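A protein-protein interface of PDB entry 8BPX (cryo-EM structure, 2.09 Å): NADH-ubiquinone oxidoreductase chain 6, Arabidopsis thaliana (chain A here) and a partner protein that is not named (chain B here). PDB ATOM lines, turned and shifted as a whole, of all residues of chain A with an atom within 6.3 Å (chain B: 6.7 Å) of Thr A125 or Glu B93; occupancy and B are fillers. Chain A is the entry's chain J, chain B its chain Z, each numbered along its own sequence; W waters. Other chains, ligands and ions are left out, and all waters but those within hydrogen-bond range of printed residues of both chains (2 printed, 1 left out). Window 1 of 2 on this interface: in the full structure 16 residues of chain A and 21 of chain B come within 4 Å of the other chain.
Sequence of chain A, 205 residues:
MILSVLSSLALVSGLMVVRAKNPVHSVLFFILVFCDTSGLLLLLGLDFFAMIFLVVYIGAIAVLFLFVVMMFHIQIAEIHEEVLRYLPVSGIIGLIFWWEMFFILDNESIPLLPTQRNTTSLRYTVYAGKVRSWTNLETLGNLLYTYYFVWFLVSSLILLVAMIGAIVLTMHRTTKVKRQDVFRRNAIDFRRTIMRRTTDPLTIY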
ATOM      1  N   SER A 121      -4.669 -17.339   3.955  1.00  0.00           N
ATOM      2  CA  SER A 121      -5.868 -16.938   4.680  1.00  0.00           C
ATOM      3  C   SER A 121      -6.945 -16.382   3.758  1.00  0.00           C
ATOM      4  O   SER A 121      -8.110 -16.315   4.159  1.00  0.00           O
ATOM      5  CB  SER A 121      -5.517 -15.904   5.746  1.00  0.00           C
ATOM      6  OG  SER A 121      -5.687 -14.590   5.248  1.00  0.00           O
ATOM      7  N   ARG A 123      -7.867 -17.836   1.003  1.00  0.00           N
ATOM      8  CA  ARG A 123      -8.569 -18.941   0.368  1.00  0.00           C
ATOM      9  C   ARG A 123      -9.984 -19.029   0.928  1.00  0.00           C
ATOM     10  O   ARG A 123     -10.171 -19.216   2.134  1.00  0.00           O
ATOM     11  CB  ARG A 123      -7.814 -20.250   0.595  1.00  0.00           C
ATOM     12  CG  ARG A 123      -7.686 -21.119  -0.646  1.00  0.00           C
ATOM     13  CD  ARG A 123      -6.399 -21.933  -0.639  1.00  0.00           C
ATOM     14  NE  ARG A 123      -5.230 -21.122  -0.957  1.00  0.00           N
ATOM     15  CZ  ARG A 123      -3.980 -21.562  -0.917  1.00  0.00           C
ATOM     16  NH1 ARG A 123      -3.696 -22.809  -0.579  1.00  0.00           N
ATOM     17  NH2 ARG A 123      -2.989 -20.730  -1.227  1.00  0.00           N
ATOM     18  N   TYR A 124     -10.977 -18.882   0.058  1.00  0.00           N
ATOM     19  CA  TYR A 124     -12.378 -18.944   0.458  1.00  0.00           C
ATOM     20  C   TYR A 124     -12.898 -20.365   0.277  1.00  0.00           C
ATOM     21  O   TYR A 124     -12.732 -20.959  -0.792  1.00  0.00           O
ATOM     22  CB  TYR A 124     -13.212 -17.960  -0.364  1.00  0.00           C
ATOM     23  CG  TYR A 124     -14.672 -17.905   0.026  1.00  0.00           C
ATOM     24  CD1 TYR A 124     -15.051 -17.717   1.350  1.00  0.00           C
ATOM     25  CD2 TYR A 124     -15.671 -18.042  -0.929  1.00  0.00           C
ATOM     26  CE1 TYR A 124     -16.378 -17.666   1.710  1.00  0.00           C
ATOM     27  CE2 TYR A 124     -17.002 -17.995  -0.576  1.00  0.00           C
ATOM     28  CZ  TYR A 124     -17.351 -17.808   0.744  1.00  0.00           C
ATOM     29  OH  TYR A 124     -18.674 -17.761   1.096  1.00  0.00           O
ATOM     30  N   THR A 125     -13.530 -20.902   1.317  1.00  0.00           N
ATOM     31  CA  THR A 125     -14.041 -22.268   1.312  1.00  0.00           C
ATOM     32  C   THR A 125     -15.556 -22.247   1.157  1.00  0.00           C
ATOM     33  O   THR A 125     -16.255 -21.600   1.942  1.00  0.00           O
ATOM     34  CB  THR A 125     -13.650 -23.003   2.593  1.00  0.00           C
ATOM     35  OG1 THR A 125     -12.233 -23.217   2.606  1.00  0.00           O
ATOM     36  CG2 THR A 125     -14.364 -24.338   2.685  1.00  0.00           C
ATOM     37  N   VAL A 126     -16.054 -22.958   0.152  1.00  0.00           N
ATOM     38  CA  VAL A 126     -17.483 -23.162  -0.055  1.00  0.00           C
ATOM     39  C   VAL A 126     -17.788 -24.602   0.326  1.00  0.00           C
ATOM     40  O   VAL A 126     -17.403 -25.537  -0.388  1.00  0.00           O
ATOM     41  CB  VAL A 126     -17.901 -22.871  -1.503  1.00  0.00           C
ATOM     42  CG1 VAL A 126     -19.412 -23.004  -1.659  1.00  0.00           C
ATOM     43  CG2 VAL A 126     -17.424 -21.495  -1.927  1.00  0.00           C
ATOM     44  N   TYR A 127     -18.479 -24.792   1.450  1.00  0.00           N
ATOM     45  CA  TYR A 127     -18.762 -26.145   1.910  1.00  0.00           C
ATOM     46  C   TYR A 127     -19.862 -26.819   1.097  1.00  0.00           C
ATOM     47  O   TYR A 127     -20.006 -28.042   1.177  1.00  0.00           O
ATOM     48  CB  TYR A 127     -19.150 -26.140   3.391  1.00  0.00           C
ATOM     49  CG  TYR A 127     -18.068 -25.703   4.352  1.00  0.00           C
ATOM     50  CD1 TYR A 127     -17.104 -26.596   4.791  1.00  0.00           C
ATOM     51  CD2 TYR A 127     -18.035 -24.406   4.852  1.00  0.00           C
ATOM     52  CE1 TYR A 127     -16.119 -26.207   5.676  1.00  0.00           C
ATOM     53  CE2 TYR A 127     -17.056 -24.006   5.740  1.00  0.00           C
ATOM     54  CZ  TYR A 127     -16.099 -24.916   6.150  1.00  0.00           C
ATOM     55  OH  TYR A 127     -15.117 -24.538   7.033  1.00  0.00           O
ATOM     56  N   LYS A 130     -18.850 -29.606  -1.038  1.00  0.00           N
ATOM     57  CA  LYS A 130     -18.150 -30.654  -0.306  1.00  0.00           C
ATOM     58  C   LYS A 130     -19.081 -31.649   0.376  1.00  0.00           C
ATOM     59  O   LYS A 130     -18.595 -32.587   1.015  1.00  0.00           O
ATOM     60  CB  LYS A 130     -17.220 -30.033   0.742  1.00  0.00           C
ATOM     61  CG  LYS A 130     -15.913 -29.499   0.197  1.00  0.00           C
ATOM     62  CD  LYS A 130     -15.211 -28.621   1.215  1.00  0.00           C
ATOM     63  CE  LYS A 130     -14.180 -27.726   0.559  1.00  0.00           C
ATOM     64  NZ  LYS A 130     -12.798 -28.177   0.855  1.00  0.00           N
ATOM     65  N   ILE B  88     -24.209 -22.931   9.303  1.00  0.00           N
ATOM     66  CA  ILE B  88     -23.397 -22.322  10.356  1.00  0.00           C
ATOM     67  C   ILE B  88     -21.915 -22.372   9.995  1.00  0.00           C
ATOM     68  O   ILE B  88     -21.170 -21.411  10.233  1.00  0.00           O
ATOM     69  CB  ILE B  88     -23.684 -22.976  11.722  1.00  0.00           C
ATOM     70  CG1 ILE B  88     -22.964 -22.197  12.826  1.00  0.00           C
ATOM     71  CG2 ILE B  88     -23.303 -24.454  11.739  1.00  0.00           C
ATOM     72  CD1 ILE B  88     -23.075 -22.810  14.188  1.00  0.00           C
ATOM     73  N   LEU B  89     -21.464 -23.477   9.397  1.00  0.00           N
ATOM     74  CA  LEU B  89     -20.081 -23.552   8.937  1.00  0.00           C
ATOM     75  C   LEU B  89     -19.804 -22.500   7.871  1.00  0.00           C
ATOM     76  O   LEU B  89     -18.764 -21.826   7.903  1.00  0.00           O
ATOM     77  CB  LEU B  89     -19.784 -24.955   8.409  1.00  0.00           C
ATOM     78  CG  LEU B  89     -19.983 -26.090   9.417  1.00  0.00           C
ATOM     79  CD1 LEU B  89     -20.022 -27.448   8.726  1.00  0.00           C
ATOM     80  CD2 LEU B  89     -18.897 -26.059  10.487  1.00  0.00           C
ATOM     81  N   GLN B  90     -20.736 -22.329   6.929  1.00  0.00           N
ATOM     82  CA  GLN B  90     -20.554 -21.323   5.890  1.00  0.00           C
ATOM     83  C   GLN B  90     -20.541 -19.914   6.475  1.00  0.00           C
ATOM     84  O   GLN B  90     -19.767 -19.067   6.030  1.00  0.00           O
ATOM     85  CB  GLN B  90     -21.647 -21.449   4.830  1.00  0.00           C
ATOM     86  CG  GLN B  90     -21.254 -20.909   3.465  1.00  0.00           C
ATOM     87  CD  GLN B  90     -19.819 -21.229   3.093  1.00  0.00           C
ATOM     88  OE1 GLN B  90     -19.478 -22.380   2.835  1.00  0.00           O
ATOM     89  NE2 GLN B  90     -18.973 -20.209   3.053  1.00  0.00           N
ATOM     90  N   ALA B  91     -21.401 -19.645   7.460  1.00  0.00           N
ATOM     91  CA  ALA B  91     -21.436 -18.320   8.077  1.00  0.00           C
ATOM     92  C   ALA B  91     -20.134 -18.016   8.806  1.00  0.00           C
ATOM     93  O   ALA B  91     -19.600 -16.902   8.709  1.00  0.00           O
ATOM     94  CB  ALA B  91     -22.622 -18.225   9.034  1.00  0.00           C
ATOM     95  N   GLU B  92     -19.609 -18.998   9.542  1.00  0.00           N
ATOM     96  CA  GLU B  92     -18.304 -18.846  10.174  1.00  0.00           C
ATOM     97  C   GLU B  92     -17.226 -18.548   9.139  1.00  0.00           C
ATOM     98  O   GLU B  92     -16.405 -17.638   9.318  1.00  0.00           O
ATOM     99  CB  GLU B  92     -17.964 -20.113  10.951  1.00  0.00           C
ATOM    100  CG  GLU B  92     -16.658 -20.065  11.700  1.00  0.00           C
ATOM    101  CD  GLU B  92     -16.365 -21.369  12.410  1.00  0.00           C
ATOM    102  OE1 GLU B  92     -16.890 -21.572  13.522  1.00  0.00           O
ATOM    103  OE2 GLU B  92     -15.608 -22.191  11.855  1.00  0.00           O
ATOM    104  N   GLU B  93     -17.217 -19.310   8.040  1.00  0.00           N
ATOM    105  CA  GLU B  93     -16.216 -19.088   7.003  1.00  0.00           C
ATOM    106  C   GLU B  93     -16.365 -17.704   6.380  1.00  0.00           C
ATOM    107  O   GLU B  93     -15.368 -17.050   6.059  1.00  0.00           O
ATOM    108  CB  GLU B  93     -16.309 -20.178   5.932  1.00  0.00           C
ATOM    109  CG  GLU B  93     -15.495 -19.892   4.675  1.00  0.00           C
ATOM    110  CD  GLU B  93     -13.987 -19.941   4.892  1.00  0.00           C
ATOM    111  OE1 GLU B  93     -13.534 -20.176   6.032  1.00  0.00           O
ATOM    112  OE2 GLU B  93     -13.248 -19.724   3.912  1.00  0.00           O
ATOM    113  N   ASP B  94     -17.605 -17.247   6.196  1.00  0.00           N
ATOM    114  CA  ASP B  94     -17.835 -15.927   5.617  1.00  0.00           C
ATOM    115  C   ASP B  94     -17.293 -14.831   6.524  1.00  0.00           C
ATOM    116  O   ASP B  94     -16.627 -13.900   6.060  1.00  0.00           O
ATOM    117  CB  ASP B  94     -19.327 -15.722   5.357  1.00  0.00           C
ATOM    118  CG  ASP B  94     -19.807 -16.430   4.106  1.00  0.00           C
ATOM    119  OD1 ASP B  94     -18.967 -17.016   3.392  1.00  0.00           O
ATOM    120  OD2 ASP B  94     -21.023 -16.387   3.831  1.00  0.00           O
ATOM    121  N   GLU B  95     -17.566 -14.928   7.827  1.00  0.00           N
ATOM    122  CA  GLU B  95     -17.031 -13.938   8.761  1.00  0.00           C
ATOM    123  C   GLU B  95     -15.505 -13.943   8.757  1.00  0.00           C
ATOM    124  O   GLU B  95     -14.867 -12.879   8.708  1.00  0.00           O
ATOM    125  CB  GLU B  95     -17.571 -14.202  10.167  1.00  0.00           C
ATOM    126  CG  GLU B  95     -18.997 -13.720  10.382  1.00  0.00           C
ATOM    127  CD  GLU B  95     -19.072 -12.247  10.723  1.00  0.00           C
ATOM    128  OE1 GLU B  95     -18.052 -11.543  10.576  1.00  0.00           O
ATOM    129  OE2 GLU B  95     -20.155 -11.789  11.146  1.00  0.00           O
ATOM    130  N   ARG B  96     -14.906 -15.138   8.781  1.00  0.00           N
ATOM    131  CA  ARG B  96     -13.450 -15.246   8.734  1.00  0.00           C
ATOM    132  C   ARG B  96     -12.880 -14.587   7.483  1.00  0.00           C
ATOM    133  O   ARG B  96     -11.929 -13.796   7.558  1.00  0.00           O
ATOM    134  CB  ARG B  96     -13.040 -16.718   8.800  1.00  0.00           C
ATOM    135  CG  ARG B  96     -11.599 -16.948   9.198  1.00  0.00           C
ATOM    136  CD  ARG B  96     -11.058 -18.239   8.599  1.00  0.00           C
ATOM    137  NE  ARG B  96     -11.380 -18.376   7.183  1.00  0.00           N
ATOM    138  CZ  ARG B  96     -10.654 -17.870   6.196  1.00  0.00           C
ATOM    139  NH1 ARG B  96      -9.550 -17.183   6.431  1.00  0.00           N
ATOM    140  NH2 ARG B  96     -11.050 -18.053   4.941  1.00  0.00           N
ATOM    141  N   PHE B  97     -13.459 -14.900   6.321  1.00  0.00           N
ATOM    142  CA  PHE B  97     -12.945 -14.348   5.076  1.00  0.00           C
ATOM    143  C   PHE B  97     -13.126 -12.839   5.018  1.00  0.00           C
ATOM    144  O   PHE B  97     -12.265 -12.135   4.489  1.00  0.00           O
ATOM    145  CB  PHE B  97     -13.618 -14.995   3.868  1.00  0.00           C
ATOM    146  CG  PHE B  97     -13.149 -14.432   2.561  1.00  0.00           C
ATOM    147  CD1 PHE B  97     -11.990 -14.904   1.968  1.00  0.00           C
ATOM    148  CD2 PHE B  97     -13.839 -13.405   1.943  1.00  0.00           C
ATOM    149  CE1 PHE B  97     -11.545 -14.379   0.772  1.00  0.00           C
ATOM    150  CE2 PHE B  97     -13.394 -12.872   0.752  1.00  0.00           C
ATOM    151  CZ  PHE B  97     -12.249 -13.363   0.164  1.00  0.00           C
ATOM    152  N   VAL B  98     -14.250 -12.328   5.520  1.00  0.00           N
ATOM    153  CA  VAL B  98     -14.474 -10.887   5.474  1.00  0.00           C
ATOM    154  C   VAL B  98     -13.450 -10.160   6.336  1.00  0.00           C
ATOM    155  O   VAL B  98     -12.880  -9.144   5.920  1.00  0.00           O
ATOM    156  CB  VAL B  98     -15.919 -10.552   5.888  1.00  0.00           C
ATOM    157  CG1 VAL B  98     -16.062  -9.067   6.158  1.00  0.00           C
ATOM    158  CG2 VAL B  98     -16.882 -10.976   4.802  1.00  0.00           C
ATOM    159  N   ASP B 141      -7.224 -28.024  -3.620  1.00  0.00           N
ATOM    160  CA  ASP B 141      -8.251 -28.616  -2.765  1.00  0.00           C
ATOM    161  C   ASP B 141      -8.040 -30.102  -2.492  1.00  0.00           C
ATOM    162  O   ASP B 141      -8.642 -30.630  -1.553  1.00  0.00           O
ATOM    163  CB  ASP B 141      -9.632 -28.409  -3.387  1.00  0.00           C
ATOM    164  CG  ASP B 141     -10.742 -28.420  -2.355  1.00  0.00           C
ATOM    165  OD1 ASP B 141     -11.250 -29.516  -2.036  1.00  0.00           O
ATOM    166  OD2 ASP B 141     -11.110 -27.331  -1.867  1.00  0.00           O
HETATM  167  O   HOH W   1     -15.922 -22.997   8.905  1.00  0.00           O
HETATM  168  O   HOH W   2     -21.310 -23.414   1.088  1.00  0.00           O
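O of Ser A121 sits at hydrogen-bond distance from NH1 of Arg B96 (2.8 Å). The backbone carbonyl oxygen (O) of Arg A123 is in hydrogen-bond range of the guanidinium group (NH2) of Arg B96 (3.2 Å). OH of Tyr A124 is in hydrogen-bond range of NE2 of Gln B90 (3.1 Å). OH of Tyr A124 lies within hydrogen-bond range of OD1 of Asp B94 (2.4 Å). NE2 of Gln B90 lies within hydrogen-bond range of O of Thr A125 (3.2 Å). The backbone NH (N) of Thr A125 lies within hydrogen-bond range of the side-chain carboxylate (OE2) of Glu B93 (2.9 Å). OE1 of Gln B90 is in hydrogen-bond range of N of Tyr A127 (3.0 Å). NZ of Lys A130 is in salt-bridge range of OD2 of Asp B141, at 3.3 Å.
The side-chain amide nitrogen of Gln B90 lies within hydrogen-bond range of the side-chain carboxylate of Asp B94 (3.2 Å). The guanidinium group (NH2) of Arg B96 is in salt-bridge range of the side-chain carboxylate (OE2) of Glu B93, 2.9 Å away.
O of Arg A123 touches OE2 of Glu B93, at 3.6 Å. Tyr A124 touches Glu B93. CD1 of Tyr A124 touches CB of Phe B97, at 3.98 Å. Val A126 touches Gln B90. Leu B89 touches Tyr A127. Glu B93 touches Tyr A127.
Printed residues of chain B within 4 Å of Val A126: Gln B90 (3.6 Å). Ala B91 touches none of the printed residues of chain A. Glu B93 touches just these residues of chain A: Arg A123, Tyr A124, Thr A125 and Tyr A127. Printed residues of chain A within 4 Å of Arg B96: Ser A121 (2.8 Å) and Arg A123 (3.2 Å). Printed residues of chain A within 4 Å of Asp B141: Lys A130 (3.3 Å). The nearest residue of chain B that does not touch Thr A125 is Arg B96 (5.2 Å). The nearest residue of chain A that does not touch Glu B93 is Val A126 (5.5 Å).
Hydrophobic or aromatic side chains of chain A within 4 Å of the printed part of chain B: Tyr A124 and Tyr A127. Printed residues of chain B that touch a printed residue of chain A: Leu B89, Gln B90, Glu B93, Asp B94, Arg B96, Phe B97 and Asp B141. Hydrophobic or aromatic side chains of chain B that line the printed part of chain A: Leu B89 and Phe B97. Among the printed residues, Asp or Glu carboxylates within 4 Å of a Lys or Arg side-chain nitrogen of the other chain: Lys A130 with Asp B141.
Water W1 lies within hydrogen-bond range of OH of Tyr A127, OE2 of Glu B92 and O of Leu B89. Water W2 lies within hydrogen-bond range of the side-chain amide oxygen (OE1) of Gln B90 and the backbone NH (N) of Tyr A127.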
